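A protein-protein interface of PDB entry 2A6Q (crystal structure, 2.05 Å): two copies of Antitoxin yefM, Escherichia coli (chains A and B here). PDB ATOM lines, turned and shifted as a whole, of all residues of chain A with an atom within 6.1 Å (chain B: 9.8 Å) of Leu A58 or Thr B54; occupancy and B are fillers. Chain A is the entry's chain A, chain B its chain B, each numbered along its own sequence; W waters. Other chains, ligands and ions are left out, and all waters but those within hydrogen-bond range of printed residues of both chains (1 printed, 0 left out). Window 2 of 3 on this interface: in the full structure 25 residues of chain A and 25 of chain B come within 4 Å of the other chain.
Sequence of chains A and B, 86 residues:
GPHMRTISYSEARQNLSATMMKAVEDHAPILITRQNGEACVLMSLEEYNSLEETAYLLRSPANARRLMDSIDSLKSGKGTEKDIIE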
ATOM      1  N   GLU A  53      16.989  12.329 -18.756  1.00  0.00           N
ATOM      2  CA  GLU A  53      16.930  12.860 -17.396  1.00  0.00           C
ATOM      3  C   GLU A  53      16.711  11.737 -16.367  1.00  0.00           C
ATOM      4  O   GLU A  53      17.234  11.795 -15.247  1.00  0.00           O
ATOM      5  CB  GLU A  53      15.802  13.886 -17.293  1.00  0.00           C
ATOM      6  CG  GLU A  53      15.651  14.534 -15.920  1.00  0.00           C
ATOM      7  CD  GLU A  53      16.856  15.376 -15.527  1.00  0.00           C
ATOM      8  OE1 GLU A  53      17.833  15.434 -16.299  1.00  0.00           O
ATOM      9  OE2 GLU A  53      16.826  15.981 -14.440  1.00  0.00           O
ATOM     10  N   THR A  54      15.954  10.714 -16.763  1.00  0.00           N
ATOM     11  CA  THR A  54      15.666   9.580 -15.887  1.00  0.00           C
ATOM     12  C   THR A  54      16.931   8.759 -15.690  1.00  0.00           C
ATOM     13  O   THR A  54      17.264   8.344 -14.572  1.00  0.00           O
ATOM     14  CB  THR A  54      14.574   8.644 -16.493  1.00  0.00           C
ATOM     15  OG1 THR A  54      13.361   9.381 -16.692  1.00  0.00           O
ATOM     16  CG2 THR A  54      14.290   7.472 -15.559  1.00  0.00           C
ATOM     17  N   ALA A  55      17.631   8.515 -16.790  1.00  0.00           N
ATOM     18  CA  ALA A  55      18.854   7.745 -16.716  1.00  0.00           C
ATOM     19  C   ALA A  55      19.873   8.516 -15.886  1.00  0.00           C
ATOM     20  O   ALA A  55      20.607   7.926 -15.101  1.00  0.00           O
ATOM     21  CB  ALA A  55      19.394   7.482 -18.117  1.00  0.00           C
ATOM     22  N   TYR A  56      19.901   9.837 -16.054  1.00  0.00           N
ATOM     23  CA  TYR A  56      20.843  10.685 -15.326  1.00  0.00           C
ATOM     24  C   TYR A  56      20.687  10.547 -13.815  1.00  0.00           C
ATOM     25  O   TYR A  56      21.671  10.406 -13.093  1.00  0.00           O
ATOM     26  CB  TYR A  56      20.670  12.158 -15.723  1.00  0.00           C
ATOM     27  CG  TYR A  56      21.426  13.113 -14.818  1.00  0.00           C
ATOM     28  CD1 TYR A  56      22.823  13.093 -14.758  1.00  0.00           C
ATOM     29  CD2 TYR A  56      20.746  13.984 -13.967  1.00  0.00           C
ATOM     30  CE1 TYR A  56      23.524  13.917 -13.863  1.00  0.00           C
ATOM     31  CE2 TYR A  56      21.428  14.798 -13.070  1.00  0.00           C
ATOM     32  CZ  TYR A  56      22.818  14.759 -13.020  1.00  0.00           C
ATOM     33  OH  TYR A  56      23.492  15.530 -12.101  1.00  0.00           O
ATOM     34  N   LEU A  57      19.443  10.574 -13.344  1.00  0.00           N
ATOM     35  CA  LEU A  57      19.161  10.464 -11.914  1.00  0.00           C
ATOM     36  C   LEU A  57      19.456   9.090 -11.325  1.00  0.00           C
ATOM     37  O   LEU A  57      19.635   8.952 -10.116  1.00  0.00           O
ATOM     38  CB  LEU A  57      17.701  10.826 -11.638  1.00  0.00           C
ATOM     39  CG  LEU A  57      17.343  12.287 -11.909  1.00  0.00           C
ATOM     40  CD1 LEU A  57      15.842  12.466 -11.926  1.00  0.00           C
ATOM     41  CD2 LEU A  57      17.986  13.163 -10.857  1.00  0.00           C
ATOM     42  N   LEU A  58      19.531   8.076 -12.175  1.00  0.00           N
ATOM     43  CA  LEU A  58      19.774   6.722 -11.690  1.00  0.00           C
ATOM     44  C   LEU A  58      21.174   6.219 -11.991  1.00  0.00           C
ATOM     45  O   LEU A  58      21.588   5.180 -11.482  1.00  0.00           O
ATOM     46  CB  LEU A  58      18.750   5.768 -12.303  1.00  0.00           C
ATOM     47  CG  LEU A  58      17.285   6.106 -12.000  1.00  0.00           C
ATOM     48  CD1 LEU A  58      16.376   5.130 -12.742  1.00  0.00           C
ATOM     49  CD2 LEU A  58      17.038   6.038 -10.509  1.00  0.00           C
ATOM     50  N   ARG A  59      21.895   6.962 -12.820  1.00  0.00           N
ATOM     51  CA  ARG A  59      23.243   6.587 -13.218  1.00  0.00           C
ATOM     52  C   ARG A  59      24.158   6.412 -12.005  1.00  0.00           C
ATOM     53  O   ARG A  59      24.938   5.463 -11.929  1.00  0.00           O
ATOM     54  CB  ARG A  59      23.790   7.661 -14.163  1.00  0.00           C
ATOM     55  CG  ARG A  59      24.589   7.124 -15.342  1.00  0.00           C
ATOM     56  CD  ARG A  59      24.676   8.177 -16.438  1.00  0.00           C
ATOM     57  NE  ARG A  59      23.776   7.894 -17.557  1.00  0.00           N
ATOM     58  CZ  ARG A  59      23.185   8.829 -18.295  1.00  0.00           C
ATOM     59  NH1 ARG A  59      23.389  10.112 -18.032  1.00  0.00           N
ATOM     60  NH2 ARG A  59      22.393   8.485 -19.298  1.00  0.00           N
ATOM     61  N   SER A  60      24.054   7.335 -11.055  1.00  0.00           N
ATOM     62  CA  SER A  60      24.864   7.282  -9.845  1.00  0.00           C
ATOM     63  C   SER A  60      24.205   6.353  -8.820  1.00  0.00           C
ATOM     64  O   SER A  60      23.131   6.655  -8.316  1.00  0.00           O
ATOM     65  CB  SER A  60      25.001   8.693  -9.260  1.00  0.00           C
ATOM     66  OG  SER A  60      25.776   8.678  -8.080  1.00  0.00           O
ATOM     67  N   PRO A  61      24.842   5.208  -8.504  1.00  0.00           N
ATOM     68  CA  PRO A  61      24.282   4.260  -7.534  1.00  0.00           C
ATOM     69  C   PRO A  61      23.830   4.909  -6.227  1.00  0.00           C
ATOM     70  O   PRO A  61      22.748   4.603  -5.717  1.00  0.00           O
ATOM     71  CB  PRO A  61      25.422   3.273  -7.318  1.00  0.00           C
ATOM     72  CG  PRO A  61      26.078   3.232  -8.674  1.00  0.00           C
ATOM     73  CD  PRO A  61      26.125   4.709  -9.035  1.00  0.00           C
ATOM     74  N   ASN A  63      22.883   7.994  -5.690  1.00  0.00           N
ATOM     75  CA  ASN A  63      21.700   8.817  -5.897  1.00  0.00           C
ATOM     76  C   ASN A  63      20.459   7.965  -6.185  1.00  0.00           C
ATOM     77  O   ASN A  63      19.355   8.305  -5.763  1.00  0.00           O
ATOM     78  CB  ASN A  63      21.913   9.774  -7.069  1.00  0.00           C
ATOM     79  CG  ASN A  63      20.967  10.944  -7.025  1.00  0.00           C
ATOM     80  OD1 ASN A  63      21.064  11.791  -6.135  1.00  0.00           O
ATOM     81  ND2 ASN A  63      20.036  11.001  -7.977  1.00  0.00           N
ATOM     82  N   ALA A  64      20.646   6.880  -6.932  1.00  0.00           N
ATOM     83  CA  ALA A  64      19.536   5.988  -7.276  1.00  0.00           C
ATOM     84  C   ALA A  64      18.960   5.387  -6.003  1.00  0.00           C
ATOM     85  O   ALA A  64      17.735   5.321  -5.823  1.00  0.00           O
ATOM     86  CB  ALA A  64      20.016   4.874  -8.208  1.00  0.00           C
ATOM     87  N   LEU A  67      17.075   8.126  -3.939  1.00  0.00           N
ATOM     88  CA  LEU A  67      15.874   8.516  -4.647  1.00  0.00           C
ATOM     89  C   LEU A  67      14.833   7.404  -4.568  1.00  0.00           C
ATOM     90  O   LEU A  67      13.645   7.675  -4.463  1.00  0.00           O
ATOM     91  CB  LEU A  67      16.215   8.841  -6.106  1.00  0.00           C
ATOM     92  CG  LEU A  67      15.233   9.687  -6.919  1.00  0.00           C
ATOM     93  CD1 LEU A  67      14.895  10.960  -6.157  1.00  0.00           C
ATOM     94  CD2 LEU A  67      15.849  10.014  -8.285  1.00  0.00           C
ATOM     95  N   MET A  68      15.272   6.150  -4.602  1.00  0.00           N
ATOM     96  CA  MET A  68      14.319   5.050  -4.534  1.00  0.00           C
ATOM     97  C   MET A  68      13.714   4.937  -3.131  1.00  0.00           C
ATOM     98  O   MET A  68      12.509   4.695  -2.987  1.00  0.00           O
ATOM     99  CB  MET A  68      14.986   3.738  -4.948  1.00  0.00           C
ATOM    100  CG  MET A  68      14.279   3.035  -6.108  1.00  0.00           C
ATOM    101  SD  MET A  68      14.020   4.084  -7.575  1.00  0.00           S
ATOM    102  CE  MET A  68      12.347   4.695  -7.274  1.00  0.00           C
ATOM    103  N   GLU B  46      22.033   0.792 -29.897  1.00  0.00           N
ATOM    104  CA  GLU B  46      22.887   0.480 -28.762  1.00  0.00           C
ATOM    105  C   GLU B  46      22.773   1.569 -27.695  1.00  0.00           C
ATOM    106  O   GLU B  46      22.566   1.271 -26.516  1.00  0.00           O
ATOM    107  CB  GLU B  46      24.345   0.338 -29.220  1.00  0.00           C
ATOM    108  CG  GLU B  46      24.628  -0.853 -30.143  1.00  0.00           C
ATOM    109  CD  GLU B  46      23.815  -0.832 -31.439  1.00  0.00           C
ATOM    110  OE1 GLU B  46      23.790   0.219 -32.123  1.00  0.00           O
ATOM    111  OE2 GLU B  46      23.207  -1.876 -31.783  1.00  0.00           O
ATOM    112  N   GLU B  47      22.908   2.831 -28.102  1.00  0.00           N
ATOM    113  CA  GLU B  47      22.803   3.919 -27.138  1.00  0.00           C
ATOM    114  C   GLU B  47      21.400   3.965 -26.546  1.00  0.00           C
ATOM    115  O   GLU B  47      21.220   4.249 -25.366  1.00  0.00           O
ATOM    116  CB  GLU B  47      23.133   5.280 -27.775  1.00  0.00           C
ATOM    117  CG  GLU B  47      23.150   6.415 -26.736  1.00  0.00           C
ATOM    118  CD  GLU B  47      23.622   7.767 -27.272  1.00  0.00           C
ATOM    119  OE1 GLU B  47      23.817   8.681 -26.445  1.00  0.00           O
ATOM    120  OE2 GLU B  47      23.793   7.930 -28.499  1.00  0.00           O
ATOM    121  N   TYR B  48      20.395   3.683 -27.367  1.00  0.00           N
ATOM    122  CA  TYR B  48      19.024   3.705 -26.872  1.00  0.00           C
ATOM    123  C   TYR B  48      18.772   2.647 -25.789  1.00  0.00           C
ATOM    124  O   TYR B  48      18.138   2.935 -24.776  1.00  0.00           O
ATOM    125  CB  TYR B  48      18.032   3.483 -28.013  1.00  0.00           C
ATOM    126  CG  TYR B  48      16.614   3.345 -27.521  1.00  0.00           C
ATOM    127  CD1 TYR B  48      15.857   4.467 -27.216  1.00  0.00           C
ATOM    128  CD2 TYR B  48      16.039   2.092 -27.327  1.00  0.00           C
ATOM    129  CE1 TYR B  48      14.560   4.351 -26.731  1.00  0.00           C
ATOM    130  CE2 TYR B  48      14.741   1.964 -26.839  1.00  0.00           C
ATOM    131  CZ  TYR B  48      14.011   3.101 -26.548  1.00  0.00           C
ATOM    132  OH  TYR B  48      12.718   2.998 -26.097  1.00  0.00           O
ATOM    133  N   ASN B  49      19.237   1.422 -26.016  1.00  0.00           N
ATOM    134  CA  ASN B  49      19.029   0.352 -25.038  1.00  0.00           C
ATOM    135  C   ASN B  49      19.787   0.608 -23.748  1.00  0.00           C
ATOM    136  O   ASN B  49      19.263   0.381 -22.652  1.00  0.00           O
ATOM    137  CB  ASN B  49      19.452  -0.998 -25.614  1.00  0.00           C
ATOM    138  CG  ASN B  49      18.483  -1.504 -26.653  1.00  0.00           C
ATOM    139  OD1 ASN B  49      17.300  -1.154 -26.625  1.00  0.00           O
ATOM    140  ND2 ASN B  49      18.963  -2.336 -27.563  1.00  0.00           N
ATOM    141  N   SER B  50      21.022   1.076 -23.888  1.00  0.00           N
ATOM    142  CA  SER B  50      21.860   1.386 -22.741  1.00  0.00           C
ATOM    143  C   SER B  50      21.128   2.397 -21.871  1.00  0.00           C
ATOM    144  O   SER B  50      21.092   2.281 -20.646  1.00  0.00           O
ATOM    145  CB  SER B  50      23.196   1.975 -23.211  1.00  0.00           C
ATOM    146  OG  SER B  50      24.060   2.209 -22.117  1.00  0.00           O
ATOM    147  N   LEU B  51      20.526   3.384 -22.523  1.00  0.00           N
ATOM    148  CA  LEU B  51      19.796   4.437 -21.836  1.00  0.00           C
ATOM    149  C   LEU B  51      18.583   3.886 -21.098  1.00  0.00           C
ATOM    150  O   LEU B  51      18.285   4.308 -19.975  1.00  0.00           O
ATOM    151  CB  LEU B  51      19.366   5.500 -22.850  1.00  0.00           C
ATOM    152  CG  LEU B  51      19.357   6.961 -22.395  1.00  0.00           C
ATOM    153  CD1 LEU B  51      20.687   7.319 -21.753  1.00  0.00           C
ATOM    154  CD2 LEU B  51      19.088   7.862 -23.598  1.00  0.00           C
ATOM    155  N   GLU B  52      17.872   2.951 -21.724  1.00  0.00           N
ATOM    156  CA  GLU B  52      16.708   2.365 -21.075  1.00  0.00           C
ATOM    157  C   GLU B  52      17.131   1.470 -19.919  1.00  0.00           C
ATOM    158  O   GLU B  52      16.489   1.470 -18.878  1.00  0.00           O
ATOM    159  CB  GLU B  52      15.862   1.563 -22.068  1.00  0.00           C
ATOM    160  CG  GLU B  52      14.561   2.253 -22.426  1.00  0.00           C
ATOM    161  CD  GLU B  52      13.515   1.295 -22.968  1.00  0.00           C
ATOM    162  OE1 GLU B  52      12.370   1.739 -23.187  1.00  0.00           O
ATOM    163  OE2 GLU B  52      13.834   0.103 -23.174  1.00  0.00           O
ATOM    164  N   GLU B  53      18.208   0.709 -20.106  1.00  0.00           N
ATOM    165  CA  GLU B  53      18.710  -0.175 -19.058  1.00  0.00           C
ATOM    166  C   GLU B  53      18.993   0.630 -17.802  1.00  0.00           C
ATOM    167  O   GLU B  53      18.735   0.174 -16.690  1.00  0.00           O
ATOM    168  CB  GLU B  53      20.007  -0.859 -19.486  1.00  0.00           C
ATOM    169  CG  GLU B  53      19.867  -1.907 -20.564  1.00  0.00           C
ATOM    170  CD  GLU B  53      21.178  -2.628 -20.808  1.00  0.00           C
ATOM    171  OE1 GLU B  53      21.645  -3.330 -19.885  1.00  0.00           O
ATOM    172  OE2 GLU B  53      21.745  -2.484 -21.914  1.00  0.00           O
ATOM    173  N   THR B  54      19.546   1.824 -17.986  1.00  0.00           N
ATOM    174  CA  THR B  54      19.859   2.692 -16.861  1.00  0.00           C
ATOM    175  C   THR B  54      18.581   3.179 -16.189  1.00  0.00           C
ATOM    176  O   THR B  54      18.416   3.038 -14.976  1.00  0.00           O
ATOM    177  CB  THR B  54      20.685   3.910 -17.305  1.00  0.00           C
ATOM    178  OG1 THR B  54      21.934   3.466 -17.850  1.00  0.00           O
ATOM    179  CG2 THR B  54      20.953   4.826 -16.125  1.00  0.00           C
ATOM    180  N   ALA B  55      17.676   3.741 -16.981  1.00  0.00           N
ATOM    181  CA  ALA B  55      16.416   4.251 -16.456  1.00  0.00           C
ATOM    182  C   ALA B  55      15.569   3.137 -15.841  1.00  0.00           C
ATOM    183  O   ALA B  55      14.556   3.400 -15.195  1.00  0.00           O
ATOM    184  CB  ALA B  55      15.640   4.952 -17.562  1.00  0.00           C
ATOM    185  N   TYR B  56      15.990   1.893 -16.050  1.00  0.00           N
ATOM    186  CA  TYR B  56      15.284   0.731 -15.512  1.00  0.00           C
ATOM    187  C   TYR B  56      15.970   0.189 -14.263  1.00  0.00           C
ATOM    188  O   TYR B  56      15.512  -0.798 -13.685  1.00  0.00           O
ATOM    189  CB  TYR B  56      15.232  -0.401 -16.540  1.00  0.00           C
ATOM    190  CG  TYR B  56      13.952  -0.493 -17.337  1.00  0.00           C
ATOM    191  CD1 TYR B  56      13.886  -0.015 -18.644  1.00  0.00           C
ATOM    192  CD2 TYR B  56      12.816  -1.088 -16.795  1.00  0.00           C
ATOM    193  CE1 TYR B  56      12.719  -0.134 -19.396  1.00  0.00           C
ATOM    194  CE2 TYR B  56      11.642  -1.210 -17.536  1.00  0.00           C
ATOM    195  CZ  TYR B  56      11.601  -0.732 -18.837  1.00  0.00           C
ATOM    196  OH  TYR B  56      10.450  -0.855 -19.581  1.00  0.00           O
ATOM    197  N   LEU B  57      17.062   0.825 -13.850  1.00  0.00           N
ATOM    198  CA  LEU B  57      17.802   0.355 -12.686  1.00  0.00           C
ATOM    199  C   LEU B  57      18.224  -1.084 -12.980  1.00  0.00           C
ATOM    200  O   LEU B  57      17.861  -2.009 -12.253  1.00  0.00           O
ATOM    201  CB  LEU B  57      16.919   0.395 -11.432  1.00  0.00           C
ATOM    202  CG  LEU B  57      16.446   1.763 -10.938  1.00  0.00           C
ATOM    203  CD1 LEU B  57      15.482   1.591  -9.772  1.00  0.00           C
ATOM    204  CD2 LEU B  57      17.647   2.590 -10.521  1.00  0.00           C
ATOM    205  N   LEU B  58      18.984  -1.256 -14.060  1.00  0.00           N
ATOM    206  CA  LEU B  58      19.468  -2.559 -14.511  1.00  0.00           C
ATOM    207  C   LEU B  58      18.342  -3.581 -14.643  1.00  0.00           C
ATOM    208  O   LEU B  58      18.052  -3.975 -15.793  1.00  0.00           O
ATOM    209  CB  LEU B  58      20.574  -3.083 -13.575  1.00  0.00           C
ATOM    210  CG  LEU B  58      20.332  -3.435 -12.102  1.00  0.00           C
ATOM    211  CD1 LEU B  58      19.779  -4.847 -11.974  1.00  0.00           C
ATOM    212  CD2 LEU B  58      21.650  -3.342 -11.344  1.00  0.00           C
HETATM  213  O   HOH W   1      23.272   5.380 -18.952  1.00  0.00           O
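Glu A53 touches none of the printed residues of chain B.
Printed residues of chain B within 4 Å of Thr A54: Ala B55.
Of the printed residues of chain B, Ala A55 touches Leu B51 and Thr B54.
No residue of chain B comes within 4 Å of Leu A57.
Leu A58 touches just these residues of chain B: Thr B54, Ala B55 and Leu B57.
Of the printed residues of chain B, Arg A59 touches Leu B51.
No residue of chain B comes within 4 Å of Ala A64.
Printed residues of chain B within 4 Å of Met A68: Leu B57.
Of the printed residues of chain A, Leu B51 touches Ala A55 (3.8 Å) and Arg A59 (3.2 Å).
Of chain A, only Ala A55 (3.3 Å) and Leu A58 (3.7 Å) come within 4 Å of Thr B54.
Printed residues of chain A within 4 Å of Ala B55: Thr A54 and Leu A58.
The nearest printed residue of chain B that does not touch Thr A54 is Thr B54 (5.3 Å).
Thr A54 touches Ala B55, and with the chains exchanged Ala A55 touches Thr B54.
Leu A58 touches Thr B54, but with the chains exchanged Thr A54 does not touch Leu B58 (9.8 Å).
Leu A58 touches Ala B55, but with the chains exchanged Ala A55 does not touch Leu B58 (9.4 Å).
Leu A58 touches Leu B57, but with the chains exchanged Leu A57 does not touch Leu B58 (10.7 Å).
Of the 13 printed residues of chain A, 5 touch a printed residue of chain B.
Among the printed residues, 8 pairs touch across the chains.
Ala B55 touches Thr A54.
Ala A55 touches Leu B51.
Thr B54 touches Ala A55.
Leu A58 touches Thr B54.
Ala B55 touches Leu A58 (O to CD1, 3.5 Å).
Leu A58 touches Leu B57.
Arg A59 touches Leu B51.
Met A68 touches Leu B57 (SD to CD1, 3.6 Å).
O of Ser B50 is in hydrogen-bond range of OG1 of Thr B54, at 3.2 Å.
Water W1 lies within hydrogen-bond range of OG1 of Thr B54 (2.6 Å) and NE of Arg A59 (2.9 Å).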
